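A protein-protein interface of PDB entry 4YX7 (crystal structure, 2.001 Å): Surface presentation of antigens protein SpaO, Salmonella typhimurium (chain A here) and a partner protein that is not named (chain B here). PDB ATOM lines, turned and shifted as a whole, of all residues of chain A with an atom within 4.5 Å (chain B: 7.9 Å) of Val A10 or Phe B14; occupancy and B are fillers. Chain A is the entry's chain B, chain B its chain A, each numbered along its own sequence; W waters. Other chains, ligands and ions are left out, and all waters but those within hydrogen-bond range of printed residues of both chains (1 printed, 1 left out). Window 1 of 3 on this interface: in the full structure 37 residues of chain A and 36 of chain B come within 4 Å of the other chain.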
ATOM      1  N   GLU A   8     -19.833 -14.260  19.842  1.00  0.00           N
ATOM      2  CA  GLU A   8     -18.485 -13.863  20.198  1.00  0.00           C
ATOM      3  C   GLU A   8     -17.526 -15.027  20.074  1.00  0.00           C
ATOM      4  O   GLU A   8     -17.870 -16.161  20.407  1.00  0.00           O
ATOM      5  CB  GLU A   8     -18.432 -13.337  21.622  1.00  0.00           C
ATOM      6  CG  GLU A   8     -18.869 -11.909  21.803  1.00  0.00           C
ATOM      7  CD  GLU A   8     -18.743 -11.488  23.247  1.00  0.00           C
ATOM      8  OE1 GLU A   8     -18.664 -12.394  24.102  1.00  0.00           O
ATOM      9  OE2 GLU A   8     -18.720 -10.272  23.530  1.00  0.00           O
ATOM     10  N   PHE A   9     -16.319 -14.734  19.606  1.00  0.00           N
ATOM     11  CA  PHE A   9     -15.263 -15.734  19.512  1.00  0.00           C
ATOM     12  C   PHE A   9     -14.219 -15.412  20.564  1.00  0.00           C
ATOM     13  O   PHE A   9     -13.537 -14.414  20.487  1.00  0.00           O
ATOM     14  CB  PHE A   9     -14.689 -15.761  18.098  1.00  0.00           C
ATOM     15  CG  PHE A   9     -15.725 -16.112  17.052  1.00  0.00           C
ATOM     16  CD1 PHE A   9     -15.990 -17.438  16.734  1.00  0.00           C
ATOM     17  CD2 PHE A   9     -16.473 -15.123  16.431  1.00  0.00           C
ATOM     18  CE1 PHE A   9     -16.951 -17.769  15.798  1.00  0.00           C
ATOM     19  CE2 PHE A   9     -17.427 -15.447  15.489  1.00  0.00           C
ATOM     20  CZ  PHE A   9     -17.668 -16.770  15.171  1.00  0.00           C
ATOM     21  N   VAL A  10     -14.140 -16.255  21.582  1.00  0.00           N
ATOM     22  CA  VAL A  10     -13.381 -15.930  22.776  1.00  0.00           C
ATOM     23  C   VAL A  10     -12.133 -16.803  22.882  1.00  0.00           C
ATOM     24  O   VAL A  10     -12.227 -18.019  23.056  1.00  0.00           O
ATOM     25  CB  VAL A  10     -14.261 -16.082  24.033  1.00  0.00           C
ATOM     26  CG1 VAL A  10     -13.501 -15.661  25.280  1.00  0.00           C
ATOM     27  CG2 VAL A  10     -15.551 -15.263  23.862  1.00  0.00           C
ATOM     28  N   LEU A  11     -10.968 -16.169  22.767  1.00  0.00           N
ATOM     29  CA  LEU A  11      -9.694 -16.881  22.815  1.00  0.00           C
ATOM     30  C   LEU A  11      -9.391 -17.394  24.215  1.00  0.00           C
ATOM     31  O   LEU A  11      -8.808 -18.458  24.369  1.00  0.00           O
ATOM     32  CB  LEU A  11      -8.549 -15.985  22.330  1.00  0.00           C
ATOM     33  CG  LEU A  11      -7.154 -16.620  22.267  1.00  0.00           C
ATOM     34  CD1 LEU A  11      -7.117 -17.744  21.256  1.00  0.00           C
ATOM     35  CD2 LEU A  11      -6.079 -15.595  21.979  1.00  0.00           C
ATOM     36  N   TYR A  12      -9.793 -16.640  25.235  1.00  0.00           N
ATOM     37  CA  TYR A  12      -9.460 -17.009  26.603  1.00  0.00           C
ATOM     38  C   TYR A  12     -10.382 -16.352  27.602  1.00  0.00           C
ATOM     39  O   TYR A  12     -10.868 -15.244  27.376  1.00  0.00           O
ATOM     40  CB  TYR A  12      -8.017 -16.627  26.916  1.00  0.00           C
ATOM     41  CG  TYR A  12      -7.467 -17.186  28.215  1.00  0.00           C
ATOM     42  CD1 TYR A  12      -7.268 -18.554  28.382  1.00  0.00           C
ATOM     43  CD2 TYR A  12      -7.104 -16.339  29.257  1.00  0.00           C
ATOM     44  CE1 TYR A  12      -6.747 -19.056  29.560  1.00  0.00           C
ATOM     45  CE2 TYR A  12      -6.586 -16.837  30.433  1.00  0.00           C
ATOM     46  CZ  TYR A  12      -6.407 -18.191  30.584  1.00  0.00           C
ATOM     47  OH  TYR A  12      -5.883 -18.677  31.770  1.00  0.00           O
ATOM     48  N   ARG A  13     -10.616 -17.050  28.707  1.00  0.00           N
ATOM     49  CA  ARG A  13     -11.383 -16.517  29.821  1.00  0.00           C
ATOM     50  C   ARG A  13     -10.620 -16.724  31.132  1.00  0.00           C
ATOM     51  O   ARG A  13      -9.903 -17.720  31.287  1.00  0.00           O
ATOM     52  CB  ARG A  13     -12.764 -17.170  29.877  1.00  0.00           C
ATOM     53  CG  ARG A  13     -13.615 -16.849  28.668  1.00  0.00           C
ATOM     54  CD  ARG A  13     -15.053 -17.195  28.905  1.00  0.00           C
ATOM     55  NE  ARG A  13     -15.261 -18.637  28.942  1.00  0.00           N
ATOM     56  CZ  ARG A  13     -16.314 -19.220  29.502  1.00  0.00           C
ATOM     57  NH1 ARG A  13     -17.251 -18.484  30.087  1.00  0.00           N
ATOM     58  NH2 ARG A  13     -16.425 -20.540  29.491  1.00  0.00           N
ATOM     59  N   MET A  24      -2.818  -6.351  35.398  1.00  0.00           N
ATOM     60  CA  MET A  24      -3.091  -6.504  33.978  1.00  0.00           C
ATOM     61  C   MET A  24      -3.250  -5.144  33.304  1.00  0.00           C
ATOM     62  O   MET A  24      -2.863  -4.963  32.148  1.00  0.00           O
ATOM     63  CB  MET A  24      -4.351  -7.338  33.797  1.00  0.00           C
ATOM     64  CG  MET A  24      -4.797  -7.560  32.384  1.00  0.00           C
ATOM     65  SD  MET A  24      -6.243  -8.621  32.461  1.00  0.00           S
ATOM     66  CE  MET A  24      -5.607  -9.919  33.516  1.00  0.00           C
ATOM     67  N   LEU A  30      -0.145 -12.026  30.335  1.00  0.00           N
ATOM     68  CA  LEU A  30      -1.053 -13.114  30.653  1.00  0.00           C
ATOM     69  C   LEU A  30      -0.711 -14.323  29.775  1.00  0.00           C
ATOM     70  O   LEU A  30      -0.874 -14.290  28.561  1.00  0.00           O
ATOM     71  CB  LEU A  30      -2.497 -12.666  30.463  1.00  0.00           C
ATOM     72  CG  LEU A  30      -3.536 -13.503  31.190  1.00  0.00           C
ATOM     73  CD1 LEU A  30      -4.728 -12.642  31.497  1.00  0.00           C
ATOM     74  CD2 LEU A  30      -3.949 -14.672  30.328  1.00  0.00           C
ATOM     75  N   VAL A  40     -10.890 -22.288  20.781  1.00  0.00           N
ATOM     76  CA  VAL A  40     -11.586 -21.011  20.803  1.00  0.00           C
ATOM     77  C   VAL A  40     -13.043 -21.253  21.219  1.00  0.00           C
ATOM     78  O   VAL A  40     -13.668 -22.191  20.742  1.00  0.00           O
ATOM     79  CB  VAL A  40     -11.507 -20.311  19.421  1.00  0.00           C
ATOM     80  CG1 VAL A  40     -12.437 -19.108  19.362  1.00  0.00           C
ATOM     81  CG2 VAL A  40     -10.077 -19.887  19.128  1.00  0.00           C
ATOM     82  N   GLU A  41     -13.575 -20.430  22.122  1.00  0.00           N
ATOM     83  CA  GLU A  41     -14.948 -20.611  22.595  1.00  0.00           C
ATOM     84  C   GLU A  41     -15.914 -19.711  21.860  1.00  0.00           C
ATOM     85  O   GLU A  41     -15.589 -18.577  21.547  1.00  0.00           O
ATOM     86  CB  GLU A  41     -15.043 -20.342  24.099  1.00  0.00           C
ATOM     87  CG  GLU A  41     -14.433 -21.424  24.957  1.00  0.00           C
ATOM     88  CD  GLU A  41     -14.436 -21.064  26.421  1.00  0.00           C
ATOM     89  OE1 GLU A  41     -13.932 -19.979  26.763  1.00  0.00           O
ATOM     90  OE2 GLU A  41     -14.943 -21.863  27.238  1.00  0.00           O
ATOM     91  N   MET A  43     -19.458 -17.816  22.081  1.00  0.00           N
ATOM     92  CA  MET A  43     -20.399 -17.353  23.086  1.00  0.00           C
ATOM     93  C   MET A  43     -21.401 -16.399  22.473  1.00  0.00           C
ATOM     94  O   MET A  43     -21.092 -15.705  21.511  1.00  0.00           O
ATOM     95  CB  MET A  43     -19.648 -16.693  24.236  1.00  0.00           C
ATOM     96  CG  MET A  43     -18.585 -17.592  24.826  1.00  0.00           C
ATOM     97  SD  MET A  43     -17.898 -16.864  26.292  1.00  0.00           S
ATOM     98  CE  MET A  43     -19.157 -17.211  27.507  1.00  0.00           C
ATOM     99  N   PRO B  11     -15.142 -11.737  35.844  1.00  0.00           N
ATOM    100  CA  PRO B  11     -14.960 -12.698  34.757  1.00  0.00           C
ATOM    101  C   PRO B  11     -14.585 -12.024  33.449  1.00  0.00           C
ATOM    102  O   PRO B  11     -15.451 -11.408  32.834  1.00  0.00           O
ATOM    103  CB  PRO B  11     -16.339 -13.353  34.649  1.00  0.00           C
ATOM    104  CG  PRO B  11     -17.267 -12.283  35.045  1.00  0.00           C
ATOM    105  CD  PRO B  11     -16.563 -11.436  36.071  1.00  0.00           C
ATOM    106  N   LEU B  12     -13.335 -12.140  33.010  1.00  0.00           N
ATOM    107  CA  LEU B  12     -12.950 -11.484  31.765  1.00  0.00           C
ATOM    108  C   LEU B  12     -13.004 -12.437  30.574  1.00  0.00           C
ATOM    109  O   LEU B  12     -12.695 -13.617  30.692  1.00  0.00           O
ATOM    110  CB  LEU B  12     -11.557 -10.879  31.883  1.00  0.00           C
ATOM    111  CG  LEU B  12     -11.298  -9.945  33.062  1.00  0.00           C
ATOM    112  CD1 LEU B  12      -9.904  -9.399  32.972  1.00  0.00           C
ATOM    113  CD2 LEU B  12     -12.303  -8.821  33.101  1.00  0.00           C
ATOM    114  N   ARG B  13     -13.436 -11.913  29.433  1.00  0.00           N
ATOM    115  CA  ARG B  13     -13.430 -12.653  28.181  1.00  0.00           C
ATOM    116  C   ARG B  13     -12.531 -11.910  27.224  1.00  0.00           C
ATOM    117  O   ARG B  13     -12.685 -10.702  27.037  1.00  0.00           O
ATOM    118  CB  ARG B  13     -14.834 -12.779  27.593  1.00  0.00           C
ATOM    119  CG  ARG B  13     -15.862 -13.334  28.547  1.00  0.00           C
ATOM    120  CD  ARG B  13     -17.135 -13.647  27.809  1.00  0.00           C
ATOM    121  NE  ARG B  13     -17.561 -12.513  27.001  1.00  0.00           N
ATOM    122  CZ  ARG B  13     -18.200 -11.458  27.495  1.00  0.00           C
ATOM    123  NH1 ARG B  13     -18.475 -11.405  28.792  1.00  0.00           N
ATOM    124  NH2 ARG B  13     -18.562 -10.454  26.701  1.00  0.00           N
ATOM    125  N   PHE B  14     -11.577 -12.617  26.635  1.00  0.00           N
ATOM    126  CA  PHE B  14     -10.705 -12.003  25.654  1.00  0.00           C
ATOM    127  C   PHE B  14     -11.211 -12.350  24.265  1.00  0.00           C
ATOM    128  O   PHE B  14     -11.014 -13.444  23.761  1.00  0.00           O
ATOM    129  CB  PHE B  14      -9.254 -12.436  25.883  1.00  0.00           C
ATOM    130  CG  PHE B  14      -8.697 -11.955  27.207  1.00  0.00           C
ATOM    131  CD1 PHE B  14      -8.878 -12.706  28.371  1.00  0.00           C
ATOM    132  CD2 PHE B  14      -8.042 -10.744  27.300  1.00  0.00           C
ATOM    133  CE1 PHE B  14      -8.396 -12.265  29.591  1.00  0.00           C
ATOM    134  CE2 PHE B  14      -7.553 -10.306  28.513  1.00  0.00           C
ATOM    135  CZ  PHE B  14      -7.730 -11.071  29.659  1.00  0.00           C
ATOM    136  N   VAL B  15     -11.893 -11.385  23.669  1.00  0.00           N
ATOM    137  CA  VAL B  15     -12.611 -11.585  22.427  1.00  0.00           C
ATOM    138  C   VAL B  15     -11.754 -11.236  21.210  1.00  0.00           C
ATOM    139  O   VAL B  15     -11.264 -10.117  21.092  1.00  0.00           O
ATOM    140  CB  VAL B  15     -13.892 -10.734  22.418  1.00  0.00           C
ATOM    141  CG1 VAL B  15     -14.726 -11.041  21.202  1.00  0.00           C
ATOM    142  CG2 VAL B  15     -14.677 -10.971  23.692  1.00  0.00           C
ATOM    143  N   ILE B  16     -11.589 -12.198  20.307  1.00  0.00           N
ATOM    144  CA  ILE B  16     -10.815 -12.002  19.081  1.00  0.00           C
ATOM    145  C   ILE B  16     -11.690 -11.757  17.853  1.00  0.00           C
ATOM    146  O   ILE B  16     -11.183 -11.551  16.754  1.00  0.00           O
ATOM    147  CB  ILE B  16      -9.911 -13.207  18.778  1.00  0.00           C
ATOM    148  CG1 ILE B  16     -10.759 -14.465  18.563  1.00  0.00           C
ATOM    149  CG2 ILE B  16      -8.890 -13.398  19.891  1.00  0.00           C
ATOM    150  CD1 ILE B  16      -9.968 -15.687  18.206  1.00  0.00           C
ATOM    151  N   GLY B  17     -13.002 -11.773  18.024  1.00  0.00           N
ATOM    152  CA  GLY B  17     -13.860 -11.489  16.898  1.00  0.00           C
ATOM    153  C   GLY B  17     -15.296 -11.821  17.176  1.00  0.00           C
ATOM    154  O   GLY B  17     -15.595 -12.462  18.180  1.00  0.00           O
ATOM    155  N   SER B  18     -16.183 -11.368  16.287  1.00  0.00           N
ATOM    156  CA  SER B  18     -17.603 -11.633  16.430  1.00  0.00           C
ATOM    157  C   SER B  18     -18.299 -11.752  15.088  1.00  0.00           C
ATOM    158  O   SER B  18     -17.780 -11.332  14.057  1.00  0.00           O
ATOM    159  CB  SER B  18     -18.275 -10.547  17.270  1.00  0.00           C
ATOM    160  OG  SER B  18     -18.291  -9.313  16.579  1.00  0.00           O
ATOM    161  N   ILE B  37     -15.576 -15.672  11.019  1.00  0.00           N
ATOM    162  CA  ILE B  37     -15.457 -14.493  11.859  1.00  0.00           C
ATOM    163  C   ILE B  37     -15.531 -13.246  10.978  1.00  0.00           C
ATOM    164  O   ILE B  37     -14.588 -12.928  10.256  1.00  0.00           O
ATOM    165  CB  ILE B  37     -14.150 -14.505  12.644  1.00  0.00           C
ATOM    166  CG1 ILE B  37     -14.046 -15.806  13.455  1.00  0.00           C
ATOM    167  CG2 ILE B  37     -14.052 -13.279  13.510  1.00  0.00           C
ATOM    168  CD1 ILE B  37     -12.892 -15.857  14.436  1.00  0.00           C
ATOM    169  N   ARG B  41     -11.937  -8.506  16.217  1.00  0.00           N
ATOM    170  CA  ARG B  41     -11.780  -7.645  17.376  1.00  0.00           C
ATOM    171  C   ARG B  41     -10.602  -8.155  18.199  1.00  0.00           C
ATOM    172  O   ARG B  41     -10.083  -9.239  17.930  1.00  0.00           O
ATOM    173  CB  ARG B  41     -13.063  -7.625  18.214  1.00  0.00           C
ATOM    174  CG  ARG B  41     -14.343  -7.704  17.393  1.00  0.00           C
ATOM    175  CD  ARG B  41     -15.599  -7.584  18.265  1.00  0.00           C
ATOM    176  NE  ARG B  41     -16.290  -6.309  18.069  1.00  0.00           N
ATOM    177  CZ  ARG B  41     -17.545  -6.183  17.649  1.00  0.00           C
ATOM    178  NH1 ARG B  41     -18.263  -7.261  17.382  1.00  0.00           N
ATOM    179  NH2 ARG B  41     -18.083  -4.977  17.499  1.00  0.00           N
ATOM    180  N   ALA B  42     -10.160  -7.362  19.170  1.00  0.00           N
ATOM    181  CA  ALA B  42      -9.203  -7.817  20.178  1.00  0.00           C
ATOM    182  C   ALA B  42      -9.504  -7.059  21.447  1.00  0.00           C
ATOM    183  O   ALA B  42      -8.743  -6.191  21.853  1.00  0.00           O
ATOM    184  CB  ALA B  42      -7.778  -7.588  19.740  1.00  0.00           C
ATOM    185  N   GLU B  43     -10.639  -7.380  22.060  1.00  0.00           N
ATOM    186  CA  GLU B  43     -11.156  -6.607  23.184  1.00  0.00           C
ATOM    187  C   GLU B  43     -11.251  -7.421  24.464  1.00  0.00           C
ATOM    188  O   GLU B  43     -11.518  -8.616  24.432  1.00  0.00           O
ATOM    189  CB  GLU B  43     -12.544  -6.048  22.866  1.00  0.00           C
ATOM    190  CG  GLU B  43     -12.674  -5.280  21.583  1.00  0.00           C
ATOM    191  CD  GLU B  43     -14.044  -5.495  20.959  1.00  0.00           C
ATOM    192  OE1 GLU B  43     -14.555  -6.634  21.049  1.00  0.00           O
ATOM    193  OE2 GLU B  43     -14.622  -4.531  20.406  1.00  0.00           O
ATOM    194  N   VAL B  44     -11.045  -6.754  25.591  1.00  0.00           N
ATOM    195  CA  VAL B  44     -11.305  -7.360  26.882  1.00  0.00           C
ATOM    196  C   VAL B  44     -12.721  -6.990  27.309  1.00  0.00           C
ATOM    197  O   VAL B  44     -13.102  -5.819  27.325  1.00  0.00           O
ATOM    198  CB  VAL B  44     -10.301  -6.910  27.952  1.00  0.00           C
ATOM    199  CG1 VAL B  44     -10.421  -7.795  29.162  1.00  0.00           C
ATOM    200  CG2 VAL B  44      -8.894  -6.947  27.408  1.00  0.00           C
ATOM    201  N   TYR B  45     -13.506  -8.010  27.625  1.00  0.00           N
ATOM    202  CA  TYR B  45     -14.865  -7.816  28.088  1.00  0.00           C
ATOM    203  C   TYR B  45     -15.025  -8.360  29.499  1.00  0.00           C
ATOM    204  O   TYR B  45     -14.425  -9.371  29.865  1.00  0.00           O
ATOM    205  CB  TYR B  45     -15.867  -8.506  27.149  1.00  0.00           C
ATOM    206  CG  TYR B  45     -16.334  -7.662  25.991  1.00  0.00           C
ATOM    207  CD1 TYR B  45     -15.510  -7.426  24.909  1.00  0.00           C
ATOM    208  CD2 TYR B  45     -17.607  -7.106  25.979  1.00  0.00           C
ATOM    209  CE1 TYR B  45     -15.932  -6.661  23.843  1.00  0.00           C
ATOM    210  CE2 TYR B  45     -18.041  -6.330  24.914  1.00  0.00           C
ATOM    211  CZ  TYR B  45     -17.195  -6.115  23.845  1.00  0.00           C
ATOM    212  OH  TYR B  45     -17.607  -5.355  22.768  1.00  0.00           O
ATOM    213  N   CYS B  46     -15.818  -7.651  30.290  1.00  0.00           N
ATOM    214  CA  CYS B  46     -16.366  -8.175  31.522  1.00  0.00           C
ATOM    215  C   CYS B  46     -17.865  -8.011  31.412  1.00  0.00           C
ATOM    216  O   CYS B  46     -18.369  -6.898  31.469  1.00  0.00           O
ATOM    217  CB  CYS B  46     -15.819  -7.438  32.740  1.00  0.00           C
ATOM    218  SG  CYS B  46     -16.231  -8.231  34.299  1.00  0.00           S
ATOM    219  N   LEU B  51     -13.659  -3.275  28.270  1.00  0.00           N
ATOM    220  CA  LEU B  51     -12.694  -2.627  29.147  1.00  0.00           C
ATOM    221  C   LEU B  51     -11.521  -1.991  28.387  1.00  0.00           C
ATOM    222  O   LEU B  51     -10.999  -0.954  28.797  1.00  0.00           O
ATOM    223  CB  LEU B  51     -12.174  -3.634  30.175  1.00  0.00           C
ATOM    224  CG  LEU B  51     -13.217  -4.409  30.983  1.00  0.00           C
ATOM    225  CD1 LEU B  51     -12.538  -5.353  31.945  1.00  0.00           C
ATOM    226  CD2 LEU B  51     -14.138  -3.464  31.737  1.00  0.00           C
ATOM    227  N   GLY B  52     -11.119  -2.609  27.280  1.00  0.00           N
ATOM    228  CA  GLY B  52      -9.984  -2.140  26.492  1.00  0.00           C
ATOM    229  C   GLY B  52      -9.529  -3.130  25.425  1.00  0.00           C
ATOM    230  O   GLY B  52     -10.198  -4.131  25.210  1.00  0.00           O
ATOM    231  N   HIS B  53      -8.409  -2.843  24.753  1.00  0.00           N
ATOM    232  CA  HIS B  53      -7.844  -3.745  23.740  1.00  0.00           C
ATOM    233  C   HIS B  53      -6.692  -4.570  24.308  1.00  0.00           C
ATOM    234  O   HIS B  53      -6.001  -4.133  25.224  1.00  0.00           O
ATOM    235  CB  HIS B  53      -7.323  -2.975  22.512  1.00  0.00           C
ATOM    236  CG  HIS B  53      -8.271  -1.952  21.969  1.00  0.00           C
ATOM    237  ND1 HIS B  53      -7.953  -0.607  21.892  1.00  0.00           N
ATOM    238  CD2 HIS B  53      -9.521  -2.066  21.459  1.00  0.00           C
ATOM    239  CE1 HIS B  53      -8.966   0.055  21.372  1.00  0.00           C
ATOM    240  NE2 HIS B  53      -9.936  -0.807  21.099  1.00  0.00           N
ATOM    241  N   PHE B  54      -6.470  -5.755  23.753  1.00  0.00           N
ATOM    242  CA  PHE B  54      -5.260  -6.504  24.065  1.00  0.00           C
ATOM    243  C   PHE B  54      -4.508  -6.842  22.783  1.00  0.00           C
ATOM    244  O   PHE B  54      -4.927  -6.477  21.680  1.00  0.00           O
ATOM    245  CB  PHE B  54      -5.579  -7.777  24.859  1.00  0.00           C
ATOM    246  CG  PHE B  54      -6.418  -8.780  24.114  1.00  0.00           C
ATOM    247  CD1 PHE B  54      -7.796  -8.741  24.192  1.00  0.00           C
ATOM    248  CD2 PHE B  54      -5.827  -9.776  23.358  1.00  0.00           C
ATOM    249  CE1 PHE B  54      -8.566  -9.656  23.517  1.00  0.00           C
ATOM    250  CE2 PHE B  54      -6.597 -10.705  22.671  1.00  0.00           C
ATOM    251  CZ  PHE B  54      -7.970 -10.648  22.756  1.00  0.00           C
ATOM    252  N   ASN B  55      -3.391  -7.541  22.930  1.00  0.00           N
ATOM    253  CA  ASN B  55      -2.633  -7.996  21.773  1.00  0.00           C
ATOM    254  C   ASN B  55      -2.057  -9.383  21.970  1.00  0.00           C
ATOM    255  O   ASN B  55      -1.494  -9.681  23.015  1.00  0.00           O
ATOM    256  CB  ASN B  55      -1.521  -7.007  21.458  1.00  0.00           C
ATOM    257  CG  ASN B  55      -2.059  -5.690  20.979  1.00  0.00           C
ATOM    258  OD1 ASN B  55      -2.867  -5.642  20.047  1.00  0.00           O
ATOM    259  ND2 ASN B  55      -1.636  -4.604  21.620  1.00  0.00           N
ATOM    260  N   ILE B  61      -0.842 -12.866  26.159  1.00  0.00           N
ATOM    261  CA  ILE B  61      -1.627 -11.655  25.909  1.00  0.00           C
ATOM    262  C   ILE B  61      -1.100 -10.459  26.718  1.00  0.00           C
ATOM    263  O   ILE B  61      -0.778 -10.589  27.901  1.00  0.00           O
ATOM    264  CB  ILE B  61      -3.132 -11.879  26.259  1.00  0.00           C
ATOM    265  CG1 ILE B  61      -3.799 -12.800  25.240  1.00  0.00           C
ATOM    266  CG2 ILE B  61      -3.884 -10.564  26.324  1.00  0.00           C
ATOM    267  CD1 ILE B  61      -5.178 -13.255  25.661  1.00  0.00           C
ATOM    268  N   ILE B  62      -0.997  -9.300  26.070  1.00  0.00           N
ATOM    269  CA  ILE B  62      -0.695  -8.048  26.762  1.00  0.00           C
ATOM    270  C   ILE B  62      -1.883  -7.113  26.624  1.00  0.00           C
ATOM    271  O   ILE B  62      -2.295  -6.809  25.512  1.00  0.00           O
ATOM    272  CB  ILE B  62       0.565  -7.351  26.196  1.00  0.00           C
ATOM    273  CG1 ILE B  62       1.795  -8.250  26.324  1.00  0.00           C
ATOM    274  CG2 ILE B  62       0.808  -6.029  26.907  1.00  0.00           C
ATOM    275  CD1 ILE B  62       2.297  -8.407  27.736  1.00  0.00           C
ATOM    276  N   VAL B  63      -2.439  -6.663  27.744  1.00  0.00           N
ATOM    277  CA  VAL B  63      -3.602  -5.776  27.698  1.00  0.00           C
ATOM    278  C   VAL B  63      -3.166  -4.313  27.795  1.00  0.00           C
ATOM    279  O   VAL B  63      -2.296  -3.982  28.598  1.00  0.00           O
ATOM    280  CB  VAL B  63      -4.610  -6.102  28.822  1.00  0.00           C
ATOM    281  CG1 VAL B  63      -5.775  -5.121  28.805  1.00  0.00           C
ATOM    282  CG2 VAL B  63      -5.125  -7.519  28.668  1.00  0.00           C
ATOM    283  N   LEU B  66      -7.747  -1.430  29.914  1.00  0.00           N
ATOM    284  CA  LEU B  66      -8.497  -1.689  31.143  1.00  0.00           C
ATOM    285  C   LEU B  66      -8.972  -0.385  31.765  1.00  0.00           C
ATOM    286  O   LEU B  66      -8.384   0.119  32.721  1.00  0.00           O
ATOM    287  CB  LEU B  66      -7.675  -2.501  32.148  1.00  0.00           C
ATOM    288  CG  LEU B  66      -7.619  -3.996  31.825  1.00  0.00           C
ATOM    289  CD1 LEU B  66      -7.027  -4.777  32.963  1.00  0.00           C
ATOM    290  CD2 LEU B  66      -8.997  -4.527  31.505  1.00  0.00           C
HETATM  291  O   HOH W   1      -1.057  -7.277  30.513  1.00  0.00           O
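Among the printed residues, merely in contact across the chains: Arg A13 with Leu B12, Phe A9 with Val B15, Val A10 with Phe B14, Leu A11 with Ile B16, Met A24 with Leu B66, Met A43 with Arg B13, Phe A9 with Ser B18, Met A24 with Val B63, Glu A8 with Gly B17, Tyr A12 with Arg B13, Met A24 with Leu B12, Leu A30 with Phe B14, Phe A9 with Ile B37, Val A10 with Arg B13 and Arg A13 with Arg B13.
Of the 24 printed residues of chain B, 11 touch a printed residue of chain A. Hydrophobic or aromatic side chains of chain B that line the printed part of chain A: Leu B12, Phe B14, Val B15, Ile B16, Ile B37, Val B63 and Leu B66. Along chain B the printed residues that touch a printed residue of chain A span positions 12 to 66. Among the printed residues, Asp or Glu carboxylates within 4 Å of a Lys or Arg side-chain nitrogen of the other chain: Glu A8 with Arg B13 (3.1 Å).
Water W1 lies within hydrogen-bond range of N of Val B63 (3.2 Å) and O of Met A24 (3.4 Å).
OE1 of Glu A8 lies within salt-bridge range of NE of Arg B13, at 3.1 Å. The backbone carbonyl oxygen (O) of Phe B14 sits at hydrogen-bond distance from the backbone NH (N) of Leu A11 (2.9 Å). O of Tyr A12 lies within hydrogen-bond range of N of Phe B14. The backbone carbonyl oxygen of Phe A9 lies within hydrogen-bond range of the backbone NH of Ile B16 (3.0 Å). The backbone carbonyl oxygen of Gly B17 is in hydrogen-bond range of the backbone NH of Phe A9, at 2.8 Å. N of Ile B61 sits at hydrogen-bond distance from O of Leu A30, 2.8 Å away.
Printed residues of chain B within 4 Å of Glu A8: Arg B13 and Gly B17. Val A10 touches just these residues of chain B: Arg B13 (3.9 Å) and Phe B14 (3.6 Å). Printed residues of chain A within 4 Å of Leu B12: Arg A13 and Met A24. Of the printed residues of chain A, Phe B14 touches Val A10 (3.6 Å), Leu A11 (2.9 Å), Tyr A12 (2.8 Å) and Leu A30 (3.9 Å). Tyr B45 touches none of the printed residues of chain A. The nearest residue of chain B that does not touch Val A10 is Val B15 (4.4 Å).
The backbone NH of Arg B13 sits at hydrogen-bond distance from the backbone carbonyl oxygen of Tyr B45, at 2.8 Å. N of Val B15 sits at hydrogen-bond distance from O of Glu B43, 2.9 Å away. The backbone carbonyl oxygen of Ile B16 sits at hydrogen-bond distance from the backbone NH of Arg B41. The backbone carbonyl oxygen (O) of Leu B51 lies within hydrogen-bond range of the backbone NH (N) of Leu B66 (3.5 Å). The backbone NH of Glu A8 sits at hydrogen-bond distance from the backbone carbonyl oxygen of Met A43. The guanidinium group (NE) of Arg A13 lies within salt-bridge range of the side-chain carboxylate (OE1) of Glu A41.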
